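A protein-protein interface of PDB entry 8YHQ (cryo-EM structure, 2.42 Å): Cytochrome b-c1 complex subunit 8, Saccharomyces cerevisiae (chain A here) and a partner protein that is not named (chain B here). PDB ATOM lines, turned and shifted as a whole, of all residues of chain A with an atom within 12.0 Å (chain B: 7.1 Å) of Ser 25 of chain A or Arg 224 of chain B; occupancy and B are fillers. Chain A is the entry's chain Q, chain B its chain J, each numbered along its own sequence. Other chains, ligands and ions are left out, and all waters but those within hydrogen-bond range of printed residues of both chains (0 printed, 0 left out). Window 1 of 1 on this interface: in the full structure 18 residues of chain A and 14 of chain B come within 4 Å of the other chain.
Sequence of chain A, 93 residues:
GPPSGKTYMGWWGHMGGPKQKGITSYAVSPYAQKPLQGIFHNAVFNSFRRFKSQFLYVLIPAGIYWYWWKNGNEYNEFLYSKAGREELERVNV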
ATOM      1  N   TRP A  12     -26.346 -16.637  17.336  1.00  0.00           N
ATOM      2  CA  TRP A  12     -25.478 -15.627  17.930  1.00  0.00           C
ATOM      3  C   TRP A  12     -25.412 -14.379  17.060  1.00  0.00           C
ATOM      4  O   TRP A  12     -24.985 -14.436  15.904  1.00  0.00           O
ATOM      5  CB  TRP A  12     -24.075 -16.201  18.137  1.00  0.00           C
ATOM      6  CG  TRP A  12     -24.019 -17.409  19.011  1.00  0.00           C
ATOM      7  CD1 TRP A  12     -23.802 -18.689  18.617  1.00  0.00           C
ATOM      8  CD2 TRP A  12     -24.178 -17.451  20.431  1.00  0.00           C
ATOM      9  NE1 TRP A  12     -23.822 -19.526  19.695  1.00  0.00           N
ATOM     10  CE2 TRP A  12     -24.050 -18.790  20.823  1.00  0.00           C
ATOM     11  CE3 TRP A  12     -24.419 -16.488  21.408  1.00  0.00           C
ATOM     12  CZ2 TRP A  12     -24.153 -19.188  22.141  1.00  0.00           C
ATOM     13  CZ3 TRP A  12     -24.521 -16.886  22.712  1.00  0.00           C
ATOM     14  CH2 TRP A  12     -24.389 -18.221  23.069  1.00  0.00           C
ATOM     15  N   GLY A  13     -25.817 -13.246  17.639  1.00  0.00           N
ATOM     16  CA  GLY A  13     -25.909 -11.976  16.954  1.00  0.00           C
ATOM     17  C   GLY A  13     -27.330 -11.538  16.664  1.00  0.00           C
ATOM     18  O   GLY A  13     -27.608 -10.333  16.668  1.00  0.00           O
ATOM     19  N   GLN A  20     -31.442  -4.233  24.379  1.00  0.00           N
ATOM     20  CA  GLN A  20     -30.963  -3.954  25.725  1.00  0.00           C
ATOM     21  C   GLN A  20     -30.122  -2.686  25.730  1.00  0.00           C
ATOM     22  O   GLN A  20     -29.345  -2.438  24.803  1.00  0.00           O
ATOM     23  CB  GLN A  20     -30.136  -5.115  26.273  1.00  0.00           C
ATOM     24  CG  GLN A  20     -30.792  -6.464  26.190  1.00  0.00           C
ATOM     25  CD  GLN A  20     -29.976  -7.549  26.853  1.00  0.00           C
ATOM     26  OE1 GLN A  20     -29.010  -7.276  27.558  1.00  0.00           O
ATOM     27  NE2 GLN A  20     -30.339  -8.791  26.599  1.00  0.00           N
ATOM     28  N   LYS A  21     -30.274  -1.901  26.791  1.00  0.00           N
ATOM     29  CA  LYS A  21     -29.522  -0.675  26.986  1.00  0.00           C
ATOM     30  C   LYS A  21     -29.457  -0.406  28.479  1.00  0.00           C
ATOM     31  O   LYS A  21     -30.475  -0.476  29.171  1.00  0.00           O
ATOM     32  CB  LYS A  21     -30.172   0.499  26.247  1.00  0.00           C
ATOM     33  CG  LYS A  21     -29.326   1.736  26.089  1.00  0.00           C
ATOM     34  CD  LYS A  21     -30.116   2.816  25.408  1.00  0.00           C
ATOM     35  CE  LYS A  21     -29.453   4.166  25.490  1.00  0.00           C
ATOM     36  NZ  LYS A  21     -28.222   4.248  24.681  1.00  0.00           N
ATOM     37  N   GLY A  22     -28.254  -0.132  28.971  1.00  0.00           N
ATOM     38  CA  GLY A  22     -28.064   0.269  30.347  1.00  0.00           C
ATOM     39  C   GLY A  22     -27.744  -0.829  31.332  1.00  0.00           C
ATOM     40  O   GLY A  22     -27.836  -0.589  32.540  1.00  0.00           O
ATOM     41  N   ILE A  23     -27.355  -2.015  30.865  1.00  0.00           N
ATOM     42  CA  ILE A  23     -26.997  -3.139  31.726  1.00  0.00           C
ATOM     43  C   ILE A  23     -25.507  -3.406  31.578  1.00  0.00           C
ATOM     44  O   ILE A  23     -24.990  -3.470  30.457  1.00  0.00           O
ATOM     45  CB  ILE A  23     -27.812  -4.405  31.402  1.00  0.00           C
ATOM     46  CG1 ILE A  23     -29.308  -4.163  31.602  1.00  0.00           C
ATOM     47  CG2 ILE A  23     -27.372  -5.548  32.300  1.00  0.00           C
ATOM     48  CD1 ILE A  23     -30.194  -5.183  30.962  1.00  0.00           C
ATOM     49  N   THR A  24     -24.827  -3.569  32.710  1.00  0.00           N
ATOM     50  CA  THR A  24     -23.402  -3.862  32.767  1.00  0.00           C
ATOM     51  C   THR A  24     -23.158  -5.169  33.514  1.00  0.00           C
ATOM     52  O   THR A  24     -23.775  -5.434  34.548  1.00  0.00           O
ATOM     53  CB  THR A  24     -22.644  -2.718  33.450  1.00  0.00           C
ATOM     54  OG1 THR A  24     -23.091  -1.470  32.923  1.00  0.00           O
ATOM     55  CG2 THR A  24     -21.145  -2.835  33.232  1.00  0.00           C
ATOM     56  N   SER A  25     -22.241  -5.978  32.976  1.00  0.00           N
ATOM     57  CA  SER A  25     -21.878  -7.281  33.525  1.00  0.00           C
ATOM     58  C   SER A  25     -20.405  -7.305  33.916  1.00  0.00           C
ATOM     59  O   SER A  25     -19.559  -6.795  33.178  1.00  0.00           O
ATOM     60  CB  SER A  25     -22.161  -8.394  32.512  1.00  0.00           C
ATOM     61  OG  SER A  25     -22.040  -9.670  33.100  1.00  0.00           O
ATOM     62  N   TYR A  26     -20.105  -7.911  35.070  1.00  0.00           N
ATOM     63  CA  TYR A  26     -18.745  -8.109  35.558  1.00  0.00           C
ATOM     64  C   TYR A  26     -18.513  -9.575  35.917  1.00  0.00           C
ATOM     65  O   TYR A  26     -19.436 -10.278  36.329  1.00  0.00           O
ATOM     66  CB  TYR A  26     -18.449  -7.260  36.799  1.00  0.00           C
ATOM     67  CG  TYR A  26     -18.827  -5.807  36.737  1.00  0.00           C
ATOM     68  CD1 TYR A  26     -20.107  -5.388  37.057  1.00  0.00           C
ATOM     69  CD2 TYR A  26     -17.892  -4.845  36.407  1.00  0.00           C
ATOM     70  CE1 TYR A  26     -20.447  -4.066  37.023  1.00  0.00           C
ATOM     71  CE2 TYR A  26     -18.224  -3.518  36.371  1.00  0.00           C
ATOM     72  CZ  TYR A  26     -19.504  -3.131  36.681  1.00  0.00           C
ATOM     73  OH  TYR A  26     -19.840  -1.805  36.645  1.00  0.00           O
ATOM     74  N   ALA A  27     -17.262 -10.022  35.788  1.00  0.00           N
ATOM     75  CA  ALA A  27     -16.894 -11.402  36.086  1.00  0.00           C
ATOM     76  C   ALA A  27     -15.402 -11.494  36.383  1.00  0.00           C
ATOM     77  O   ALA A  27     -14.625 -10.606  36.030  1.00  0.00           O
ATOM     78  CB  ALA A  27     -17.256 -12.340  34.935  1.00  0.00           C
ATOM     79  N   VAL A  28     -15.016 -12.597  37.038  1.00  0.00           N
ATOM     80  CA  VAL A  28     -13.631 -12.896  37.396  1.00  0.00           C
ATOM     81  C   VAL A  28     -13.282 -14.297  36.903  1.00  0.00           C
ATOM     82  O   VAL A  28     -14.138 -15.183  36.825  1.00  0.00           O
ATOM     83  CB  VAL A  28     -13.392 -12.769  38.921  1.00  0.00           C
ATOM     84  CG1 VAL A  28     -11.986 -13.174  39.291  1.00  0.00           C
ATOM     85  CG2 VAL A  28     -13.640 -11.356  39.387  1.00  0.00           C
ATOM     86  N   SER A  29     -12.010 -14.490  36.569  1.00  0.00           N
ATOM     87  CA  SER A  29     -11.548 -15.757  36.023  1.00  0.00           C
ATOM     88  C   SER A  29     -11.651 -16.870  37.066  1.00  0.00           C
ATOM     89  O   SER A  29     -11.497 -16.609  38.263  1.00  0.00           O
ATOM     90  CB  SER A  29     -10.101 -15.640  35.559  1.00  0.00           C
ATOM     91  OG  SER A  29      -9.652 -16.830  34.953  1.00  0.00           O
ATOM     92  N   PRO A  30     -11.880 -18.123  36.654  1.00  0.00           N
ATOM     93  CA  PRO A  30     -11.864 -19.217  37.635  1.00  0.00           C
ATOM     94  C   PRO A  30     -10.477 -19.585  38.125  1.00  0.00           C
ATOM     95  O   PRO A  30     -10.339 -20.019  39.273  1.00  0.00           O
ATOM     96  CB  PRO A  30     -12.517 -20.374  36.870  1.00  0.00           C
ATOM     97  CG  PRO A  30     -12.280 -20.091  35.500  1.00  0.00           C
ATOM     98  CD  PRO A  30     -12.332 -18.615  35.343  1.00  0.00           C
ATOM     99  N   GLU B 222     -13.479  -9.379  33.337  1.00  0.00           N
ATOM    100  CA  GLU B 222     -14.115  -8.740  32.194  1.00  0.00           C
ATOM    101  C   GLU B 222     -15.195  -7.781  32.667  1.00  0.00           C
ATOM    102  O   GLU B 222     -15.736  -7.912  33.766  1.00  0.00           O
ATOM    103  CB  GLU B 222     -14.705  -9.766  31.222  1.00  0.00           C
ATOM    104  CG  GLU B 222     -15.648 -10.758  31.838  1.00  0.00           C
ATOM    105  CD  GLU B 222     -16.332 -11.621  30.812  1.00  0.00           C
ATOM    106  OE1 GLU B 222     -15.892 -11.620  29.645  1.00  0.00           O
ATOM    107  OE2 GLU B 222     -17.315 -12.301  31.172  1.00  0.00           O
ATOM    108  N   VAL B 223     -15.494  -6.804  31.813  1.00  0.00           N
ATOM    109  CA  VAL B 223     -16.604  -5.878  32.018  1.00  0.00           C
ATOM    110  C   VAL B 223     -17.267  -5.622  30.672  1.00  0.00           C
ATOM    111  O   VAL B 223     -16.594  -5.287  29.693  1.00  0.00           O
ATOM    112  CB  VAL B 223     -16.159  -4.560  32.689  1.00  0.00           C
ATOM    113  CG1 VAL B 223     -15.070  -3.851  31.910  1.00  0.00           C
ATOM    114  CG2 VAL B 223     -17.336  -3.645  32.907  1.00  0.00           C
ATOM    115  N   ARG B 224     -18.588  -5.797  30.627  1.00  0.00           N
ATOM    116  CA  ARG B 224     -19.382  -5.704  29.407  1.00  0.00           C
ATOM    117  C   ARG B 224     -20.396  -4.578  29.549  1.00  0.00           C
ATOM    118  O   ARG B 224     -21.185  -4.572  30.498  1.00  0.00           O
ATOM    119  CB  ARG B 224     -20.100  -7.021  29.120  1.00  0.00           C
ATOM    120  CG  ARG B 224     -19.213  -8.179  28.758  1.00  0.00           C
ATOM    121  CD  ARG B 224     -19.973  -9.485  28.788  1.00  0.00           C
ATOM    122  NE  ARG B 224     -19.090 -10.641  28.662  1.00  0.00           N
ATOM    123  CZ  ARG B 224     -18.845 -11.324  27.547  1.00  0.00           C
ATOM    124  NH1 ARG B 224     -18.018 -12.350  27.595  1.00  0.00           N
ATOM    125  NH2 ARG B 224     -19.399 -11.007  26.386  1.00  0.00           N
ATOM    126  N   LEU B 225     -20.391  -3.646  28.596  1.00  0.00           N
ATOM    127  CA  LEU B 225     -21.266  -2.471  28.593  1.00  0.00           C
ATOM    128  C   LEU B 225     -22.111  -2.510  27.323  1.00  0.00           C
ATOM    129  O   LEU B 225     -21.780  -1.884  26.316  1.00  0.00           O
ATOM    130  CB  LEU B 225     -20.464  -1.182  28.678  1.00  0.00           C
ATOM    131  CG  LEU B 225     -19.662  -0.934  29.945  1.00  0.00           C
ATOM    132  CD1 LEU B 225     -18.211  -1.238  29.700  1.00  0.00           C
ATOM    133  CD2 LEU B 225     -19.824   0.476  30.416  1.00  0.00           C
ATOM    134  N   ARG B 226     -23.233  -3.205  27.396  1.00  0.00           N
ATOM    135  CA  ARG B 226     -24.014  -3.568  26.227  1.00  0.00           C
ATOM    136  C   ARG B 226     -24.964  -2.445  25.820  1.00  0.00           C
ATOM    137  O   ARG B 226     -25.716  -1.927  26.650  1.00  0.00           O
ATOM    138  CB  ARG B 226     -24.787  -4.840  26.546  1.00  0.00           C
ATOM    139  CG  ARG B 226     -25.631  -5.424  25.459  1.00  0.00           C
ATOM    140  CD  ARG B 226     -26.240  -6.686  25.991  1.00  0.00           C
ATOM    141  NE  ARG B 226     -27.254  -7.259  25.119  1.00  0.00           N
ATOM    142  CZ  ARG B 226     -26.997  -7.857  23.966  1.00  0.00           C
ATOM    143  NH1 ARG B 226     -27.996  -8.357  23.259  1.00  0.00           N
ATOM    144  NH2 ARG B 226     -25.756  -7.942  23.514  1.00  0.00           N
ATOM    145  N   ILE B 407     -10.601  -8.187  29.569  1.00  0.00           N
ATOM    146  CA  ILE B 407     -11.436  -7.917  28.403  1.00  0.00           C
ATOM    147  C   ILE B 407     -12.404  -6.795  28.748  1.00  0.00           C
ATOM    148  O   ILE B 407     -12.933  -6.738  29.860  1.00  0.00           O
ATOM    149  CB  ILE B 407     -12.228  -9.160  27.924  1.00  0.00           C
ATOM    150  CG1 ILE B 407     -11.414 -10.456  28.018  1.00  0.00           C
ATOM    151  CG2 ILE B 407     -12.704  -8.959  26.487  1.00  0.00           C
ATOM    152  CD1 ILE B 407     -12.205 -11.683  27.755  1.00  0.00           C
ATOM    153  N   ALA B 408     -12.635  -5.900  27.791  1.00  0.00           N
ATOM    154  CA  ALA B 408     -13.681  -4.894  27.897  1.00  0.00           C
ATOM    155  C   ALA B 408     -14.317  -4.686  26.533  1.00  0.00           C
ATOM    156  O   ALA B 408     -13.659  -4.811  25.499  1.00  0.00           O
ATOM    157  CB  ALA B 408     -13.152  -3.569  28.435  1.00  0.00           C
ATOM    158  N   GLY B 409     -15.609  -4.377  26.543  1.00  0.00           N
ATOM    159  CA  GLY B 409     -16.353  -4.234  25.308  1.00  0.00           C
ATOM    160  C   GLY B 409     -17.594  -3.394  25.480  1.00  0.00           C
ATOM    161  O   GLY B 409     -18.169  -3.322  26.569  1.00  0.00           O
ATOM    162  N   THR B 410     -18.009  -2.754  24.389  1.00  0.00           N
ATOM    163  CA  THR B 410     -19.260  -2.012  24.362  1.00  0.00           C
ATOM    164  C   THR B 410     -19.881  -2.083  22.977  1.00  0.00           C
ATOM    165  O   THR B 410     -19.201  -2.283  21.969  1.00  0.00           O
ATOM    166  CB  THR B 410     -19.090  -0.540  24.778  1.00  0.00           C
ATOM    167  OG1 THR B 410     -20.373   0.020  25.070  1.00  0.00           O
ATOM    168  CG2 THR B 410     -18.429   0.289  23.689  1.00  0.00           C
ATOM    169  N   ILE B 413     -22.376  -6.598  21.283  1.00  0.00           N
ATOM    170  CA  ILE B 413     -21.420  -7.621  21.700  1.00  0.00           C
ATOM    171  C   ILE B 413     -22.128  -8.893  22.165  1.00  0.00           C
ATOM    172  O   ILE B 413     -21.589  -9.651  22.978  1.00  0.00           O
ATOM    173  CB  ILE B 413     -20.485  -7.077  22.800  1.00  0.00           C
ATOM    174  CG1 ILE B 413     -21.271  -6.399  23.924  1.00  0.00           C
ATOM    175  CG2 ILE B 413     -19.508  -6.115  22.217  1.00  0.00           C
ATOM    176  CD1 ILE B 413     -20.515  -6.232  25.194  1.00  0.00           C
ATOM    177  N   GLU B 414     -23.337  -9.137  21.653  1.00  0.00           N
ATOM    178  CA  GLU B 414     -24.007 -10.417  21.870  1.00  0.00           C
ATOM    179  C   GLU B 414     -23.153 -11.593  21.419  1.00  0.00           C
ATOM    180  O   GLU B 414     -23.120 -12.629  22.090  1.00  0.00           O
ATOM    181  CB  GLU B 414     -25.339 -10.447  21.127  1.00  0.00           C
ATOM    182  CG  GLU B 414     -26.325 -11.451  21.662  1.00  0.00           C
ATOM    183  CD  GLU B 414     -27.450 -11.732  20.695  1.00  0.00           C
ATOM    184  OE1 GLU B 414     -28.520 -11.103  20.823  1.00  0.00           O
ATOM    185  OE2 GLU B 414     -27.263 -12.583  19.804  1.00  0.00           O
ATOM    186  N   GLY B 415     -22.478 -11.465  20.285  1.00  0.00           N
ATOM    187  CA  GLY B 415     -21.647 -12.514  19.748  1.00  0.00           C
ATOM    188  C   GLY B 415     -20.312 -12.717  20.419  1.00  0.00           C
ATOM    189  O   GLY B 415     -19.559 -13.601  20.007  1.00  0.00           O
ATOM    190  N   LEU B 416     -19.984 -11.925  21.434  1.00  0.00           N
ATOM    191  CA  LEU B 416     -18.773 -12.137  22.210  1.00  0.00           C
ATOM    192  C   LEU B 416     -19.039 -13.219  23.243  1.00  0.00           C
ATOM    193  O   LEU B 416     -19.913 -13.065  24.101  1.00  0.00           O
ATOM    194  CB  LEU B 416     -18.332 -10.838  22.875  1.00  0.00           C
ATOM    195  CG  LEU B 416     -17.017 -10.811  23.646  1.00  0.00           C
ATOM    196  CD1 LEU B 416     -15.851 -11.047  22.747  1.00  0.00           C
ATOM    197  CD2 LEU B 416     -16.867  -9.497  24.354  1.00  0.00           C
ATOM    198  N   LEU B 417     -18.295 -14.315  23.156  1.00  0.00           N
ATOM    199  CA  LEU B 417     -18.564 -15.466  23.994  1.00  0.00           C
ATOM    200  C   LEU B 417     -17.984 -15.268  25.392  1.00  0.00           C
ATOM    201  O   LEU B 417     -17.317 -14.275  25.692  1.00  0.00           O
ATOM    202  CB  LEU B 417     -18.012 -16.732  23.343  1.00  0.00           C
ATOM    203  CG  LEU B 417     -18.570 -17.110  21.970  1.00  0.00           C
ATOM    204  CD1 LEU B 417     -17.932 -18.386  21.480  1.00  0.00           C
ATOM    205  CD2 LEU B 417     -20.084 -17.250  21.981  1.00  0.00           C
ATOM    206  N   ASP B 418     -18.265 -16.239  26.251  1.00  0.00           N
ATOM    207  CA  ASP B 418     -17.929 -16.181  27.663  1.00  0.00           C
ATOM    208  C   ASP B 418     -16.417 -16.144  27.875  1.00  0.00           C
ATOM    209  O   ASP B 418     -15.617 -16.335  26.956  1.00  0.00           O
ATOM    210  CB  ASP B 418     -18.537 -17.375  28.382  1.00  0.00           C
ATOM    211  CG  ASP B 418     -18.058 -18.693  27.813  1.00  0.00           C
ATOM    212  OD1 ASP B 418     -18.642 -19.153  26.814  1.00  0.00           O
ATOM    213  OD2 ASP B 418     -17.087 -19.261  28.351  1.00  0.00           O
ATOM    214  N   TYR B 419     -16.034 -15.909  29.133  1.00  0.00           N
ATOM    215  CA  TYR B 419     -14.631 -15.727  29.489  1.00  0.00           C
ATOM    216  C   TYR B 419     -13.808 -16.976  29.197  1.00  0.00           C
ATOM    217  O   TYR B 419     -12.724 -16.889  28.611  1.00  0.00           O
ATOM    218  CB  TYR B 419     -14.515 -15.335  30.968  1.00  0.00           C
ATOM    219  CG  TYR B 419     -13.107 -15.035  31.424  1.00  0.00           C
ATOM    220  CD1 TYR B 419     -12.587 -13.760  31.339  1.00  0.00           C
ATOM    221  CD2 TYR B 419     -12.297 -16.030  31.942  1.00  0.00           C
ATOM    222  CE1 TYR B 419     -11.311 -13.490  31.744  1.00  0.00           C
ATOM    223  CE2 TYR B 419     -11.025 -15.768  32.343  1.00  0.00           C
ATOM    224  CZ  TYR B 419     -10.533 -14.500  32.244  1.00  0.00           C
ATOM    225  OH  TYR B 419      -9.255 -14.243  32.654  1.00  0.00           O
ATOM    226  N   ILE B 422     -12.624 -17.924  25.696  1.00  0.00           N
ATOM    227  CA  ILE B 422     -11.574 -17.048  25.201  1.00  0.00           C
ATOM    228  C   ILE B 422     -10.260 -17.346  25.914  1.00  0.00           C
ATOM    229  O   ILE B 422      -9.190 -17.344  25.299  1.00  0.00           O
ATOM    230  CB  ILE B 422     -12.012 -15.576  25.362  1.00  0.00           C
ATOM    231  CG1 ILE B 422     -13.254 -15.270  24.513  1.00  0.00           C
ATOM    232  CG2 ILE B 422     -10.916 -14.639  24.960  1.00  0.00           C
ATOM    233  CD1 ILE B 422     -14.051 -14.097  24.977  1.00  0.00           C
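NE of Arg 226 of chain B is in hydrogen-bond range of OE1 of Gln 20 of chain A (3.0 Å). OE2 of Glu 414 of chain B sits at hydrogen-bond distance from N of Gly 13 of chain A, 2.7 Å away. N of Glu 222 of chain B lies within hydrogen-bond range of O of Ala 27 of chain A (3.2 Å). The side-chain hydroxyl of Ser 29 of chain A sits close to the side-chain hydroxyl of Tyr 419 of chain B. The backbone carbonyl oxygen (O) of Ser 25 of chain A lies within hydrogen-bond range of the backbone NH (N) of Arg 224 of chain B (2.9 Å).
OE1 of Glu 222 of chain B lies within salt-bridge range of NH1 of Arg 224 of chain B, at 3.0 Å. The backbone carbonyl oxygen (O) of Val 223 of chain B lies within hydrogen-bond range of the backbone NH (N) of Gly 409 of chain B (3.4 Å). N of Val 223 of chain B sits at hydrogen-bond distance from O of Ile 407 of chain B (3.2 Å). The backbone carbonyl oxygen (O) of Leu 416 of chain B sits at hydrogen-bond distance from the guanidinium group (NH2) of Arg 224 of chain B (3.1 Å). The guanidinium group (NH1) of Arg 226 of chain B lies within salt-bridge range of the side-chain carboxylate (OE1) of Glu 414 of chain B, at 3.7 Å. The guanidinium group (NH1) of Arg 224 of chain B sits at hydrogen-bond distance from the backbone carbonyl oxygen (O) of Leu 417 of chain B (2.8 Å).
OE2 of Glu 414 of chain B touches C of Trp 12 of chain A, 3.8 Å away. Gly 22 of chain A touches Arg 226 of chain B. Ile 23 of chain A touches Arg 224 of chain B (O to O, 3.96 Å). N of Arg 226 of chain B touches O of Ile 23 of chain A, at 3.5 Å. Thr 24 of chain A touches Val 223 of chain B. CG2 of Thr 24 of chain A touches O of Arg 224 of chain B (3.2 Å). Val 223 of chain B touches Ser 25 of chain A. Tyr 26 of chain A touches Glu 222 of chain B. Val 223 of chain B touches Tyr 26 of chain A.
Of the printed residues of chain B, Gly 13 of chain A touches Glu 414 (2.7 Å). Of the printed residues of chain B, Gln 20 of chain A touches Arg 226. Lys 21 of chain A touches none of the printed residues of chain B. Ser 25 of chain A touches just these residues of chain B: Val 223 and Arg 224. Of the printed residues of chain B, Ser 29 of chain A touches Tyr 419. Glu 222 of chain B touches just these residues of chain A: Tyr 26 and Ala 27. Printed residues of chain A within 4 Å of Val 223 of chain B: Thr 24, Ser 25 and Tyr 26. Of chain A, only Ile 23 (3.96 Å), Thr 24 (3.2 Å) and Ser 25 (2.9 Å) come within 4 Å of Arg 224 of chain B. No residue of chain A comes within 4 Å of Leu 225 of chain B. No residue of chain A comes within 4 Å of Gly 409 of chain B. Thr 410 of chain B touches none of the printed residues of chain A. No residue of chain A comes within 4 Å of Ile 413 of chain B. Printed residues of chain A within 4 Å of Glu 414 of chain B: Trp 12 and Gly 13. No residue of chain A comes within 4 Å of Gly 415 of chain B. No residue of chain A comes within 4 Å of Leu 416 of chain B. No residue of chain A comes within 4 Å of Asp 418 of chain B. The nearest residue of chain B that does not touch Ser 25 of chain A is Glu 222 of chain B (4.03 Å). The nearest residue of chain A that does not touch Arg 224 of chain B is Tyr 26 of chain A (5.1 Å). The nearest printed residue of chain B that does not touch Gly 22 of chain A is Leu 225 of chain B (6.8 Å).
Hydrophobic or aromatic side chains of chain A that line the printed part of chain B: Tyr 26 and Ala 27. Among the printed residues, 14 pairs touch across the chains.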
